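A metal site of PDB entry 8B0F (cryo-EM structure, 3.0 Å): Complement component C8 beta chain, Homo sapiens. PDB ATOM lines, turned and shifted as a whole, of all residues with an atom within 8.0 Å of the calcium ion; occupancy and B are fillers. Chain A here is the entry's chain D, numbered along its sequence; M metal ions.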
ATOM      1  N   VAL A 134      10.808  22.506  -3.496  1.00  0.00           N
ATOM      2  CA  VAL A 134       9.929  22.806  -4.622  1.00  0.00           C
ATOM      3  C   VAL A 134       8.890  21.715  -4.767  1.00  0.00           C
ATOM      4  O   VAL A 134       9.157  20.534  -4.522  1.00  0.00           O
ATOM      5  CB  VAL A 134      10.736  22.990  -5.919  1.00  0.00           C
ATOM      6  CG1 VAL A 134      11.640  24.202  -5.820  1.00  0.00           C
ATOM      7  CG2 VAL A 134      11.532  21.742  -6.254  1.00  0.00           C
ATOM      8  N   ASN A 135       7.689  22.104  -5.185  1.00  0.00           N
ATOM      9  CA  ASN A 135       6.655  21.127  -5.498  1.00  0.00           C
ATOM     10  C   ASN A 135       7.085  20.201  -6.632  1.00  0.00           C
ATOM     11  O   ASN A 135       7.680  20.624  -7.618  1.00  0.00           O
ATOM     12  CB  ASN A 135       5.351  21.830  -5.877  1.00  0.00           C
ATOM     13  CG  ASN A 135       4.808  22.686  -4.759  1.00  0.00           C
ATOM     14  OD1 ASN A 135       4.579  22.207  -3.656  1.00  0.00           O
ATOM     15  ND2 ASN A 135       4.601  23.968  -5.047  1.00  0.00           N
ATOM     16  N   ARG A 136       6.767  18.911  -6.456  1.00  0.00           N
ATOM     17  CA  ARG A 136       7.168  17.881  -7.413  1.00  0.00           C
ATOM     18  C   ARG A 136       6.714  18.179  -8.838  1.00  0.00           C
ATOM     19  O   ARG A 136       7.342  17.734  -9.798  1.00  0.00           O
ATOM     20  CB  ARG A 136       6.618  16.532  -6.945  1.00  0.00           C
ATOM     21  CG  ARG A 136       7.318  15.335  -7.535  1.00  0.00           C
ATOM     22  CD  ARG A 136       6.762  14.058  -6.952  1.00  0.00           C
ATOM     23  NE  ARG A 136       7.025  13.963  -5.524  1.00  0.00           N
ATOM     24  CZ  ARG A 136       8.124  13.443  -4.983  1.00  0.00           C
ATOM     25  NH1 ARG A 136       9.053  12.878  -5.733  1.00  0.00           N
ATOM     26  NH2 ARG A 136       8.284  13.477  -3.663  1.00  0.00           N
ATOM     27  N   ARG A 137       5.614  18.931  -8.980  1.00  0.00           N
ATOM     28  CA  ARG A 137       5.100  19.314 -10.292  1.00  0.00           C
ATOM     29  C   ARG A 137       6.007  20.270 -11.054  1.00  0.00           C
ATOM     30  O   ARG A 137       5.850  20.416 -12.268  1.00  0.00           O
ATOM     31  CB  ARG A 137       3.708  19.936 -10.146  1.00  0.00           C
ATOM     32  CG  ARG A 137       3.729  21.391  -9.738  1.00  0.00           C
ATOM     33  CD  ARG A 137       2.349  21.897  -9.383  1.00  0.00           C
ATOM     34  NE  ARG A 137       2.302  23.344  -9.348  1.00  0.00           N
ATOM     35  CZ  ARG A 137       2.048  24.123 -10.400  1.00  0.00           C
ATOM     36  NH1 ARG A 137       1.717  23.610 -11.572  1.00  0.00           N
ATOM     37  NH2 ARG A 137       2.075  25.441 -10.249  1.00  0.00           N
ATOM     38  N   LEU A 138       6.918  20.953 -10.368  1.00  0.00           N
ATOM     39  CA  LEU A 138       7.744  21.977 -10.993  1.00  0.00           C
ATOM     40  C   LEU A 138       9.015  21.421 -11.628  1.00  0.00           C
ATOM     41  O   LEU A 138       9.771  22.185 -12.231  1.00  0.00           O
ATOM     42  CB  LEU A 138       8.122  23.043  -9.963  1.00  0.00           C
ATOM     43  CG  LEU A 138       6.950  23.785  -9.310  1.00  0.00           C
ATOM     44  CD1 LEU A 138       7.472  24.833  -8.345  1.00  0.00           C
ATOM     45  CD2 LEU A 138       6.057  24.420 -10.356  1.00  0.00           C
ATOM     46  N   LEU A 139       9.277  20.128 -11.491  1.00  0.00           N
ATOM     47  CA  LEU A 139      10.395  19.518 -12.196  1.00  0.00           C
ATOM     48  C   LEU A 139      10.146  19.520 -13.702  1.00  0.00           C
ATOM     49  O   LEU A 139       9.043  19.202 -14.159  1.00  0.00           O
ATOM     50  CB  LEU A 139      10.606  18.092 -11.714  1.00  0.00           C
ATOM     51  CG  LEU A 139      10.719  17.873 -10.208  1.00  0.00           C
ATOM     52  CD1 LEU A 139      11.030  16.422  -9.910  1.00  0.00           C
ATOM     53  CD2 LEU A 139      11.762  18.787  -9.602  1.00  0.00           C
ATOM     54  N   CYS A 140      11.173  19.864 -14.473  1.00  0.00           N
ATOM     55  CA  CYS A 140      11.163  19.698 -15.917  1.00  0.00           C
ATOM     56  C   CYS A 140      10.098  20.557 -16.599  1.00  0.00           C
ATOM     57  O   CYS A 140       9.620  20.225 -17.681  1.00  0.00           O
ATOM     58  CB  CYS A 140      11.003  18.233 -16.302  1.00  0.00           C
ATOM     59  SG  CYS A 140      12.042  17.177 -15.294  1.00  0.00           S
ATOM     60  N   ASN A 141       9.721  21.663 -15.965  1.00  0.00           N
ATOM     61  CA  ASN A 141       8.784  22.614 -16.536  1.00  0.00           C
ATOM     62  C   ASN A 141       9.498  23.666 -17.379  1.00  0.00           C
ATOM     63  O   ASN A 141       8.829  24.498 -17.997  1.00  0.00           O
ATOM     64  CB  ASN A 141       7.954  23.276 -15.434  1.00  0.00           C
ATOM     65  CG  ASN A 141       8.803  24.013 -14.438  1.00  0.00           C
ATOM     66  OD1 ASN A 141      10.024  24.027 -14.521  1.00  0.00           O
ATOM     67  ND2 ASN A 141       8.147  24.632 -13.464  1.00  0.00           N
ATOM     68  N   GLY A 142      10.822  23.639 -17.413  1.00  0.00           N
ATOM     69  CA  GLY A 142      11.617  24.622 -18.117  1.00  0.00           C
ATOM     70  C   GLY A 142      11.992  25.849 -17.315  1.00  0.00           C
ATOM     71  O   GLY A 142      12.631  26.753 -17.857  1.00  0.00           O
ATOM     72  N   ASP A 143      11.626  25.896 -16.030  1.00  0.00           N
ATOM     73  CA  ASP A 143      11.989  27.005 -15.152  1.00  0.00           C
ATOM     74  C   ASP A 143      12.962  26.501 -14.107  1.00  0.00           C
ATOM     75  O   ASP A 143      12.812  25.389 -13.584  1.00  0.00           O
ATOM     76  CB  ASP A 143      10.750  27.594 -14.470  1.00  0.00           C
ATOM     77  CG  ASP A 143       9.799  28.222 -15.454  1.00  0.00           C
ATOM     78  OD1 ASP A 143      10.243  29.048 -16.283  1.00  0.00           O
ATOM     79  OD2 ASP A 143       8.594  27.907 -15.396  1.00  0.00           O
ATOM     80  N   ASN A 144      13.958  27.317 -13.784  1.00  0.00           N
ATOM     81  CA  ASN A 144      14.857  27.030 -12.660  1.00  0.00           C
ATOM     82  C   ASN A 144      14.135  27.407 -11.377  1.00  0.00           C
ATOM     83  O   ASN A 144      14.266  28.523 -10.871  1.00  0.00           O
ATOM     84  CB  ASN A 144      16.171  27.776 -12.816  1.00  0.00           C
ATOM     85  CG  ASN A 144      17.067  27.609 -11.609  1.00  0.00           C
ATOM     86  OD1 ASN A 144      17.718  26.574 -11.445  1.00  0.00           O
ATOM     87  ND2 ASN A 144      17.105  28.619 -10.746  1.00  0.00           N
ATOM     88  N   ASP A 145      13.354  26.469 -10.856  1.00  0.00           N
ATOM     89  CA  ASP A 145      12.610  26.709  -9.621  1.00  0.00           C
ATOM     90  C   ASP A 145      13.426  26.417  -8.381  1.00  0.00           C
ATOM     91  O   ASP A 145      13.190  27.019  -7.333  1.00  0.00           O
ATOM     92  CB  ASP A 145      11.345  25.855  -9.605  1.00  0.00           C
ATOM     93  CG  ASP A 145      10.481  26.066 -10.831  1.00  0.00           C
ATOM     94  OD1 ASP A 145       9.981  27.196 -11.028  1.00  0.00           O
ATOM     95  OD2 ASP A 145      10.302  25.103 -11.607  1.00  0.00           O
ATOM     96  N   CYS A 146      14.377  25.492  -8.468  1.00  0.00           N
ATOM     97  CA  CYS A 146      15.447  25.375  -7.491  1.00  0.00           C
ATOM     98  C   CYS A 146      16.546  26.403  -7.790  1.00  0.00           C
ATOM     99  O   CYS A 146      16.376  27.324  -8.588  1.00  0.00           O
ATOM    100  CB  CYS A 146      15.999  23.959  -7.502  1.00  0.00           C
ATOM    101  SG  CYS A 146      14.925  22.736  -6.753  1.00  0.00           S
ATOM    102  N   GLN A 149      19.423  24.699 -11.366  1.00  0.00           N
ATOM    103  CA  GLN A 149      18.594  23.828 -12.194  1.00  0.00           C
ATOM    104  C   GLN A 149      18.453  22.408 -11.633  1.00  0.00           C
ATOM    105  O   GLN A 149      18.233  21.459 -12.385  1.00  0.00           O
ATOM    106  CB  GLN A 149      19.142  23.759 -13.625  1.00  0.00           C
ATOM    107  CG  GLN A 149      19.335  25.117 -14.280  1.00  0.00           C
ATOM    108  CD  GLN A 149      20.694  25.714 -13.979  1.00  0.00           C
ATOM    109  OE1 GLN A 149      21.728  25.166 -14.372  1.00  0.00           O
ATOM    110  NE2 GLN A 149      20.708  26.837 -13.275  1.00  0.00           N
ATOM    111  N   SER A 150      18.576  22.249 -10.312  1.00  0.00           N
ATOM    112  CA  SER A 150      18.567  20.913  -9.737  1.00  0.00           C
ATOM    113  C   SER A 150      17.225  20.217  -9.949  1.00  0.00           C
ATOM    114  O   SER A 150      17.152  18.994  -9.828  1.00  0.00           O
ATOM    115  CB  SER A 150      18.889  20.969  -8.243  1.00  0.00           C
ATOM    116  OG  SER A 150      18.045  21.886  -7.577  1.00  0.00           O
ATOM    117  N   ASP A 151      16.177  20.976 -10.266  1.00  0.00           N
ATOM    118  CA  ASP A 151      14.888  20.407 -10.657  1.00  0.00           C
ATOM    119  C   ASP A 151      14.795  20.108 -12.146  1.00  0.00           C
ATOM    120  O   ASP A 151      13.964  19.277 -12.546  1.00  0.00           O
ATOM    121  CB  ASP A 151      13.746  21.356 -10.275  1.00  0.00           C
ATOM    122  CG  ASP A 151      13.952  22.764 -10.804  1.00  0.00           C
ATOM    123  OD1 ASP A 151      15.101  23.219 -10.827  1.00  0.00           O
ATOM    124  OD2 ASP A 151      12.948  23.395 -11.196  1.00  0.00           O
ATOM    125  N   GLU A 152      15.618  20.737 -12.978  1.00  0.00           N
ATOM    126  CA  GLU A 152      15.609  20.513 -14.409  1.00  0.00           C
ATOM    127  C   GLU A 152      16.708  19.564 -14.878  1.00  0.00           C
ATOM    128  O   GLU A 152      16.637  19.075 -16.007  1.00  0.00           O
ATOM    129  CB  GLU A 152      15.771  21.844 -15.155  1.00  0.00           C
ATOM    130  CG  GLU A 152      14.753  22.919 -14.797  1.00  0.00           C
ATOM    131  CD  GLU A 152      13.325  22.442 -14.903  1.00  0.00           C
ATOM    132  OE1 GLU A 152      12.811  22.331 -16.031  1.00  0.00           O
ATOM    133  OE2 GLU A 152      12.701  22.197 -13.848  1.00  0.00           O
ATOM    134  N   ALA A 153      17.708  19.324 -14.039  1.00  0.00           N
ATOM    135  CA  ALA A 153      18.708  18.291 -14.342  1.00  0.00           C
ATOM    136  C   ALA A 153      18.082  16.907 -14.461  1.00  0.00           C
ATOM    137  O   ALA A 153      17.162  16.545 -13.727  1.00  0.00           O
ATOM    138  CB  ALA A 153      19.783  18.287 -13.257  1.00  0.00           C
ATOM    139  N   CYS A 155      16.137  15.694 -16.578  1.00  0.00           N
ATOM    140  CA  CYS A 155      14.799  15.583 -17.141  1.00  0.00           C
ATOM    141  C   CYS A 155      14.788  14.774 -18.430  1.00  0.00           C
ATOM    142  O   CYS A 155      15.417  15.161 -19.421  1.00  0.00           O
ATOM    143  CB  CYS A 155      14.197  16.970 -17.362  1.00  0.00           C
ATOM    144  SG  CYS A 155      13.897  17.826 -15.812  1.00  0.00           S
ATOM    145  N   ILE A 158      11.514  18.095 -21.168  1.00  0.00           N
ATOM    146  CA  ILE A 158      11.196  19.408 -20.614  1.00  0.00           C
ATOM    147  C   ILE A 158       9.932  19.943 -21.277  1.00  0.00           C
ATOM    148  O   ILE A 158       9.905  20.144 -22.500  1.00  0.00           O
ATOM    149  CB  ILE A 158      12.360  20.398 -20.782  1.00  0.00           C
ATOM    150  CG1 ILE A 158      13.617  19.832 -20.111  1.00  0.00           C
ATOM    151  CG2 ILE A 158      12.008  21.753 -20.190  1.00  0.00           C
ATOM    152  CD1 ILE A 158      14.861  20.645 -20.356  1.00  0.00           C
ATOM    153  N   TYR A 195      10.901  33.363  -8.731  1.00  0.00           N
ATOM    154  CA  TYR A 195      10.249  32.077  -8.645  1.00  0.00           C
ATOM    155  C   TYR A 195       8.821  32.230  -9.171  1.00  0.00           C
ATOM    156  O   TYR A 195       8.054  33.038  -8.653  1.00  0.00           O
ATOM    157  CB  TYR A 195      10.241  31.589  -7.196  1.00  0.00           C
ATOM    158  CG  TYR A 195       9.373  30.389  -6.927  1.00  0.00           C
ATOM    159  CD1 TYR A 195       9.753  29.123  -7.332  1.00  0.00           C
ATOM    160  CD2 TYR A 195       8.165  30.526  -6.257  1.00  0.00           C
ATOM    161  CE1 TYR A 195       8.954  28.030  -7.090  1.00  0.00           C
ATOM    162  CE2 TYR A 195       7.361  29.433  -6.006  1.00  0.00           C
ATOM    163  CZ  TYR A 195       7.766  28.190  -6.412  1.00  0.00           C
ATOM    164  OH  TYR A 195       6.978  27.098  -6.142  1.00  0.00           O
ATOM    165  N   ALA A 197       6.696  29.368 -10.032  1.00  0.00           N
ATOM    166  CA  ALA A 197       5.976  28.111 -10.077  1.00  0.00           C
ATOM    167  C   ALA A 197       5.573  27.738 -11.509  1.00  0.00           C
ATOM    168  O   ALA A 197       6.441  27.605 -12.381  1.00  0.00           O
ATOM    169  CB  ALA A 197       4.750  28.173  -9.171  1.00  0.00           C
HETATM  170 CA    CA M   1      11.433  23.580 -12.823  1.00  0.00          CA
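The calcium ion is bound by the side-chain carboxylate (OE2) of Glu 152 (2.1 Å), the side-chain carboxylate (OD2) of Asp 151 (2.2 Å), the backbone carbonyl oxygen (O) of Leu 138 (2.2 Å), the side-chain amide oxygen (OD1) of Asn 141 (2.3 Å), the side-chain carboxylate (OD2) of Asp 145 (2.3 Å) and the backbone carbonyl oxygen (O) of Asp 143 (2.4 Å).
The calcium ion has six donor atoms within binding distance.
The backbone carbonyl oxygen (O) of Asp 151 sits at hydrogen-bond distance from the backbone NH (N) of Cys 140, at 3.4 Å.
The side-chain carboxylate (OE1) of Glu 152 is in hydrogen-bond range of the backbone NH (N) of Gly 142, at 2.8 Å.
The side-chain sulfur (SG) of Cys 155 forms a disulfide with the side-chain sulfur (SG) of Cys 140, 2.0 Å away.
The backbone NH (N) of Cys 140 lies close to the side-chain carboxylate (OE1) of Glu 152, 3.3 Å away.
The side-chain carboxylate of Asp 151 lies within hydrogen-bond range of the backbone NH of Cys 146, at 3.4 Å.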
